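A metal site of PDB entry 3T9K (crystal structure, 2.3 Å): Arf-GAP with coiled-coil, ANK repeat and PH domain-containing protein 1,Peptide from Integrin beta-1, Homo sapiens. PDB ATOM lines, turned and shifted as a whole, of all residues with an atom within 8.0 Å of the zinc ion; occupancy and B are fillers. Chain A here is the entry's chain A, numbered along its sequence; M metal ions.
The side-chain sulfur of Cys 68 lies close to the backbone NH of Gln 70 (3.7 Å). The backbone carbonyl oxygen (O) of Cys 68 sits close to the side-chain hydroxyl (OG) of Ser 72, at 3.2 Å. SG of Cys 51 lies close to N of Glu 53. The side-chain amino group of Lys 134 sits close to the side-chain sulfur of Cys 51 (3.5 Å). The backbone NH (N) of Cys 48 lies within hydrogen-bond range of the backbone carbonyl oxygen (O) of Glu 53 (2.7 Å). The backbone NH of Asp 50 lies close to the side-chain sulfur of Cys 48 (3.3 Å). O of Cys 71 is in hydrogen-bond range of ND1 of His 75, at 3.0 Å.
SG of Cys 68 binds the zinc ion, 2.3 Å away. The zinc ion is bound by SG of Cys 51 (2.3 Å). The zinc ion is bound by SG of Cys 48, 2.3 Å away. SG of Cys 71 binds the zinc ion (2.4 Å). The zinc ion has four donor atoms within binding distance.
Four residues have an atom within 4 Å of the zinc ion: Cys 48, Cys 51, Cys 68 and Cys 71. The nearest printed residue that does not touch the zinc ion is Glu 53 (4.4 Å).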
ATOM      1  N   GLN A  47      -6.186   3.910 -20.867  1.00  0.00           N
ATOM      2  CA  GLN A  47      -5.009   3.264 -21.432  1.00  0.00           C
ATOM      3  C   GLN A  47      -5.250   2.862 -22.891  1.00  0.00           C
ATOM      4  O   GLN A  47      -6.395   2.676 -23.284  1.00  0.00           O
ATOM      5  CB  GLN A  47      -4.602   2.069 -20.594  1.00  0.00           C
ATOM      6  CG  GLN A  47      -5.612   0.972 -20.630  1.00  0.00           C
ATOM      7  CD  GLN A  47      -5.888   0.501 -19.244  1.00  0.00           C
ATOM      8  OE1 GLN A  47      -6.977   0.000 -18.942  1.00  0.00           O
ATOM      9  NE2 GLN A  47      -4.924   0.710 -18.378  1.00  0.00           N
ATOM     10  N   CYS A  48      -4.184   2.727 -23.672  1.00  0.00           N
ATOM     11  CA  CYS A  48      -4.300   2.439 -25.108  1.00  0.00           C
ATOM     12  C   CYS A  48      -5.061   1.138 -25.323  1.00  0.00           C
ATOM     13  O   CYS A  48      -4.835   0.156 -24.616  1.00  0.00           O
ATOM     14  CB  CYS A  48      -2.934   2.355 -25.783  1.00  0.00           C
ATOM     15  SG  CYS A  48      -2.997   1.935 -27.572  1.00  0.00           S
ATOM     16  N   CYS A  49      -5.991   1.158 -26.281  1.00  0.00           N
ATOM     17  CA  CYS A  49      -6.751  -0.045 -26.608  1.00  0.00           C
ATOM     18  C   CYS A  49      -5.846  -1.230 -27.013  1.00  0.00           C
ATOM     19  O   CYS A  49      -6.225  -2.371 -26.817  1.00  0.00           O
ATOM     20  CB  CYS A  49      -7.747   0.241 -27.729  1.00  0.00           C
ATOM     21  SG  CYS A  49      -8.858  -1.156 -28.104  1.00  0.00           S
ATOM     22  N   ASP A  50      -4.679  -0.936 -27.570  1.00  0.00           N
ATOM     23  CA  ASP A  50      -3.882  -1.965 -28.226  1.00  0.00           C
ATOM     24  C   ASP A  50      -2.624  -2.382 -27.474  1.00  0.00           C
ATOM     25  O   ASP A  50      -2.185  -3.515 -27.604  1.00  0.00           O
ATOM     26  CB  ASP A  50      -3.528  -1.562 -29.661  1.00  0.00           C
ATOM     27  CG  ASP A  50      -4.768  -1.461 -30.573  1.00  0.00           C
ATOM     28  OD1 ASP A  50      -5.812  -2.106 -30.340  1.00  0.00           O
ATOM     29  OD2 ASP A  50      -4.657  -0.723 -31.575  1.00  0.00           O
ATOM     30  N   CYS A  51      -2.052  -1.477 -26.671  1.00  0.00           N
ATOM     31  CA  CYS A  51      -0.853  -1.762 -25.873  1.00  0.00           C
ATOM     32  C   CYS A  51      -0.958  -1.308 -24.408  1.00  0.00           C
ATOM     33  O   CYS A  51       0.004  -1.442 -23.647  1.00  0.00           O
ATOM     34  CB  CYS A  51       0.363  -1.112 -26.514  1.00  0.00           C
ATOM     35  SG  CYS A  51       0.448   0.657 -26.258  1.00  0.00           S
ATOM     36  N   ARG A  52      -2.111  -0.763 -24.017  1.00  0.00           N
ATOM     37  CA  ARG A  52      -2.353  -0.321 -22.616  1.00  0.00           C
ATOM     38  C   ARG A  52      -1.528   0.887 -22.169  1.00  0.00           C
ATOM     39  O   ARG A  52      -1.483   1.181 -20.984  1.00  0.00           O
ATOM     40  CB  ARG A  52      -2.176  -1.450 -21.585  1.00  0.00           C
ATOM     41  CG  ARG A  52      -2.840  -2.788 -21.915  1.00  0.00           C
ATOM     42  CD  ARG A  52      -3.191  -3.634 -20.636  1.00  0.00           C
ATOM     43  NE  ARG A  52      -4.643  -3.782 -20.623  1.00  0.00           N
ATOM     44  CZ  ARG A  52      -5.472  -3.474 -19.643  1.00  0.00           C
ATOM     45  NH1 ARG A  52      -6.771  -3.616 -19.853  1.00  0.00           N
ATOM     46  NH2 ARG A  52      -5.014  -3.076 -18.446  1.00  0.00           N
ATOM     47  N   GLU A  53      -0.861   1.558 -23.093  1.00  0.00           N
ATOM     48  CA  GLU A  53      -0.099   2.765 -22.785  1.00  0.00           C
ATOM     49  C   GLU A  53      -1.019   3.816 -22.164  1.00  0.00           C
ATOM     50  O   GLU A  53      -2.109   4.073 -22.692  1.00  0.00           O
ATOM     51  CB  GLU A  53       0.554   3.309 -24.065  1.00  0.00           C
ATOM     52  CG  GLU A  53       1.181   4.676 -23.916  1.00  0.00           C
ATOM     53  CD  GLU A  53       2.624   4.602 -23.466  1.00  0.00           C
ATOM     54  OE1 GLU A  53       2.977   5.305 -22.487  1.00  0.00           O
ATOM     55  OE2 GLU A  53       3.420   3.877 -24.107  1.00  0.00           O
ATOM     56  N   PRO A  54      -0.620   4.385 -21.016  1.00  0.00           N
ATOM     57  CA  PRO A  54      -1.475   5.291 -20.237  1.00  0.00           C
ATOM     58  C   PRO A  54      -1.763   6.618 -20.925  1.00  0.00           C
ATOM     59  O   PRO A  54      -0.937   7.093 -21.684  1.00  0.00           O
ATOM     60  CB  PRO A  54      -0.653   5.530 -18.964  1.00  0.00           C
ATOM     61  CG  PRO A  54       0.241   4.356 -18.855  1.00  0.00           C
ATOM     62  CD  PRO A  54       0.594   3.992 -20.251  1.00  0.00           C
ATOM     63  N   PRO A  56      -3.926   7.850 -23.435  1.00  0.00           N
ATOM     64  CA  PRO A  56      -3.923   7.970 -24.907  1.00  0.00           C
ATOM     65  C   PRO A  56      -4.668   9.223 -25.399  1.00  0.00           C
ATOM     66  O   PRO A  56      -5.729   9.563 -24.881  1.00  0.00           O
ATOM     67  CB  PRO A  56      -4.682   6.701 -25.351  1.00  0.00           C
ATOM     68  CG  PRO A  56      -5.634   6.420 -24.201  1.00  0.00           C
ATOM     69  CD  PRO A  56      -4.784   6.745 -22.969  1.00  0.00           C
ATOM     70  N   THR A  66      -9.705   4.457 -27.843  1.00  0.00           N
ATOM     71  CA  THR A  66      -8.606   5.416 -27.687  1.00  0.00           C
ATOM     72  C   THR A  66      -7.297   4.707 -27.907  1.00  0.00           C
ATOM     73  O   THR A  66      -7.192   3.493 -27.711  1.00  0.00           O
ATOM     74  CB  THR A  66      -8.585   6.026 -26.302  1.00  0.00           C
ATOM     75  OG1 THR A  66      -8.533   4.967 -25.337  1.00  0.00           O
ATOM     76  CG2 THR A  66      -9.851   6.836 -26.056  1.00  0.00           C
ATOM     77  N   LEU A  67      -6.287   5.477 -28.301  1.00  0.00           N
ATOM     78  CA  LEU A  67      -5.043   4.913 -28.741  1.00  0.00           C
ATOM     79  C   LEU A  67      -3.918   5.872 -28.408  1.00  0.00           C
ATOM     80  O   LEU A  67      -4.133   7.087 -28.387  1.00  0.00           O
ATOM     81  CB  LEU A  67      -5.083   4.717 -30.264  1.00  0.00           C
ATOM     82  CG  LEU A  67      -6.168   3.807 -30.829  1.00  0.00           C
ATOM     83  CD1 LEU A  67      -6.336   4.069 -32.324  1.00  0.00           C
ATOM     84  CD2 LEU A  67      -5.777   2.361 -30.569  1.00  0.00           C
ATOM     85  N   CYS A  68      -2.730   5.312 -28.164  1.00  0.00           N
ATOM     86  CA  CYS A  68      -1.535   6.114 -27.952  1.00  0.00           C
ATOM     87  C   CYS A  68      -0.998   6.621 -29.300  1.00  0.00           C
ATOM     88  O   CYS A  68      -1.551   6.300 -30.355  1.00  0.00           O
ATOM     89  CB  CYS A  68      -0.455   5.299 -27.228  1.00  0.00           C
ATOM     90  SG  CYS A  68       0.221   3.846 -28.128  1.00  0.00           S
ATOM     91  N   ILE A  69       0.057   7.406 -29.256  1.00  0.00           N
ATOM     92  CA  ILE A  69       0.665   7.965 -30.424  1.00  0.00           C
ATOM     93  C   ILE A  69       1.177   6.853 -31.334  1.00  0.00           C
ATOM     94  O   ILE A  69       0.886   6.867 -32.543  1.00  0.00           O
ATOM     95  CB  ILE A  69       1.812   8.900 -30.033  1.00  0.00           C
ATOM     96  CG1 ILE A  69       1.276  10.070 -29.184  1.00  0.00           C
ATOM     97  CG2 ILE A  69       2.615   9.361 -31.299  1.00  0.00           C
ATOM     98  CD1 ILE A  69       2.403  10.946 -28.520  1.00  0.00           C
ATOM     99  N   GLN A  70       1.907   5.886 -30.761  1.00  0.00           N
ATOM    100  CA  GLN A  70       2.455   4.764 -31.538  1.00  0.00           C
ATOM    101  C   GLN A  70       1.375   3.925 -32.241  1.00  0.00           C
ATOM    102  O   GLN A  70       1.422   3.742 -33.457  1.00  0.00           O
ATOM    103  CB  GLN A  70       3.351   3.869 -30.680  1.00  0.00           C
ATOM    104  CG  GLN A  70       4.272   2.957 -31.517  1.00  0.00           C
ATOM    105  CD  GLN A  70       5.432   2.383 -30.724  1.00  0.00           C
ATOM    106  OE1 GLN A  70       6.575   2.292 -31.212  1.00  0.00           O
ATOM    107  NE2 GLN A  70       5.158   1.975 -29.499  1.00  0.00           N
ATOM    108  N   CYS A  71       0.382   3.436 -31.488  1.00  0.00           N
ATOM    109  CA  CYS A  71      -0.662   2.626 -32.080  1.00  0.00           C
ATOM    110  C   CYS A  71      -1.567   3.377 -33.072  1.00  0.00           C
ATOM    111  O   CYS A  71      -2.012   2.781 -34.065  1.00  0.00           O
ATOM    112  CB  CYS A  71      -1.469   1.891 -31.006  1.00  0.00           C
ATOM    113  SG  CYS A  71      -0.447   0.713 -30.118  1.00  0.00           S
ATOM    114  N   SER A  72      -1.847   4.663 -32.814  1.00  0.00           N
ATOM    115  CA  SER A  72      -2.598   5.487 -33.789  1.00  0.00           C
ATOM    116  C   SER A  72      -1.828   5.530 -35.128  1.00  0.00           C
ATOM    117  O   SER A  72      -2.441   5.447 -36.187  1.00  0.00           O
ATOM    118  CB  SER A  72      -2.815   6.915 -33.260  1.00  0.00           C
ATOM    119  OG  SER A  72      -1.588   7.656 -33.306  1.00  0.00           O
ATOM    120  N   ILE A  74       0.136   3.211 -36.284  1.00  0.00           N
ATOM    121  CA  ILE A  74      -0.063   1.894 -36.923  1.00  0.00           C
ATOM    122  C   ILE A  74      -1.475   1.796 -37.563  1.00  0.00           C
ATOM    123  O   ILE A  74      -1.623   1.272 -38.692  1.00  0.00           O
ATOM    124  CB  ILE A  74       0.239   0.717 -35.945  1.00  0.00           C
ATOM    125  CG1 ILE A  74       1.744   0.651 -35.632  1.00  0.00           C
ATOM    126  CG2 ILE A  74      -0.185  -0.625 -36.544  1.00  0.00           C
ATOM    127  CD1 ILE A  74       2.079  -0.027 -34.307  1.00  0.00           C
ATOM    128  N   HIS A  75      -2.490   2.310 -36.870  1.00  0.00           N
ATOM    129  CA  HIS A  75      -3.825   2.407 -37.441  1.00  0.00           C
ATOM    130  C   HIS A  75      -3.898   3.142 -38.785  1.00  0.00           C
ATOM    131  O   HIS A  75      -4.646   2.715 -39.652  1.00  0.00           O
ATOM    132  CB  HIS A  75      -4.831   3.041 -36.486  1.00  0.00           C
ATOM    133  CG  HIS A  75      -5.405   2.080 -35.506  1.00  0.00           C
ATOM    134  ND1 HIS A  75      -4.650   1.447 -34.541  1.00  0.00           N
ATOM    135  CD2 HIS A  75      -6.670   1.640 -35.337  1.00  0.00           C
ATOM    136  CE1 HIS A  75      -5.423   0.661 -33.825  1.00  0.00           C
ATOM    137  NE2 HIS A  75      -6.658   0.756 -34.276  1.00  0.00           N
ATOM    138  N   LYS A 124      -0.742 -10.032 -25.441  1.00  0.00           N
ATOM    139  CA  LYS A 124      -1.015  -8.662 -25.852  1.00  0.00           C
ATOM    140  C   LYS A 124       0.227  -7.790 -25.560  1.00  0.00           C
ATOM    141  O   LYS A 124       0.818  -7.908 -24.485  1.00  0.00           O
ATOM    142  CB  LYS A 124      -2.254  -8.136 -25.143  1.00  0.00           C
ATOM    143  CG  LYS A 124      -2.492  -6.661 -25.272  1.00  0.00           C
ATOM    144  CD  LYS A 124      -3.839  -6.252 -24.761  1.00  0.00           C
ATOM    145  CE  LYS A 124      -4.115  -4.803 -25.134  1.00  0.00           C
ATOM    146  NZ  LYS A 124      -5.590  -4.491 -25.218  1.00  0.00           N
ATOM    147  N   PRO A 125       0.627  -6.950 -26.518  1.00  0.00           N
ATOM    148  CA  PRO A 125       1.828  -6.134 -26.313  1.00  0.00           C
ATOM    149  C   PRO A 125       1.620  -5.148 -25.161  1.00  0.00           C
ATOM    150  O   PRO A 125       0.507  -4.646 -24.981  1.00  0.00           O
ATOM    151  CB  PRO A 125       1.983  -5.370 -27.654  1.00  0.00           C
ATOM    152  CG  PRO A 125       0.626  -5.393 -28.273  1.00  0.00           C
ATOM    153  CD  PRO A 125      -0.031  -6.657 -27.806  1.00  0.00           C
ATOM    154  N   GLY A 126       2.673  -4.903 -24.403  1.00  0.00           N
ATOM    155  CA  GLY A 126       2.668  -3.847 -23.405  1.00  0.00           C
ATOM    156  C   GLY A 126       3.230  -2.552 -23.965  1.00  0.00           C
ATOM    157  O   GLY A 126       3.675  -2.505 -25.112  1.00  0.00           O
ATOM    158  N   PRO A 127       3.213  -1.480 -23.139  1.00  0.00           N
ATOM    159  CA  PRO A 127       3.608  -0.131 -23.536  1.00  0.00           C
ATOM    160  C   PRO A 127       4.991  -0.013 -24.197  1.00  0.00           C
ATOM    161  O   PRO A 127       5.145   0.719 -25.186  1.00  0.00           O
ATOM    162  CB  PRO A 127       3.590   0.626 -22.203  1.00  0.00           C
ATOM    163  CG  PRO A 127       2.502  -0.034 -21.453  1.00  0.00           C
ATOM    164  CD  PRO A 127       2.698  -1.502 -21.756  1.00  0.00           C
ATOM    165  N   LYS A 134       3.748  -4.399 -31.990  1.00  0.00           N
ATOM    166  CA  LYS A 134       2.440  -3.769 -31.992  1.00  0.00           C
ATOM    167  C   LYS A 134       1.828  -3.797 -33.398  1.00  0.00           C
ATOM    168  O   LYS A 134       0.641  -4.039 -33.529  1.00  0.00           O
ATOM    169  CB  LYS A 134       2.513  -2.349 -31.423  1.00  0.00           C
ATOM    170  CG  LYS A 134       2.901  -2.307 -29.938  1.00  0.00           C
ATOM    171  CD  LYS A 134       3.032  -0.872 -29.495  1.00  0.00           C
ATOM    172  CE  LYS A 134       3.710  -0.741 -28.143  1.00  0.00           C
ATOM    173  NZ  LYS A 134       3.710   0.655 -27.605  1.00  0.00           N
ATOM    174  N   ILE A 138      -1.873  -5.484 -33.896  1.00  0.00           N
ATOM    175  CA  ILE A 138      -2.917  -4.643 -34.500  1.00  0.00           C
ATOM    176  C   ILE A 138      -3.463  -5.247 -35.800  1.00  0.00           C
ATOM    177  O   ILE A 138      -4.676  -5.308 -36.006  1.00  0.00           O
ATOM    178  CB  ILE A 138      -2.410  -3.200 -34.673  1.00  0.00           C
ATOM    179  CG1 ILE A 138      -2.322  -2.540 -33.292  1.00  0.00           C
ATOM    180  CG2 ILE A 138      -3.303  -2.389 -35.610  1.00  0.00           C
ATOM    181  CD1 ILE A 138      -1.558  -1.226 -33.258  1.00  0.00           C
HETATM  182 ZN    ZN M   1      -0.713   1.721 -27.971  1.00  0.00          ZN
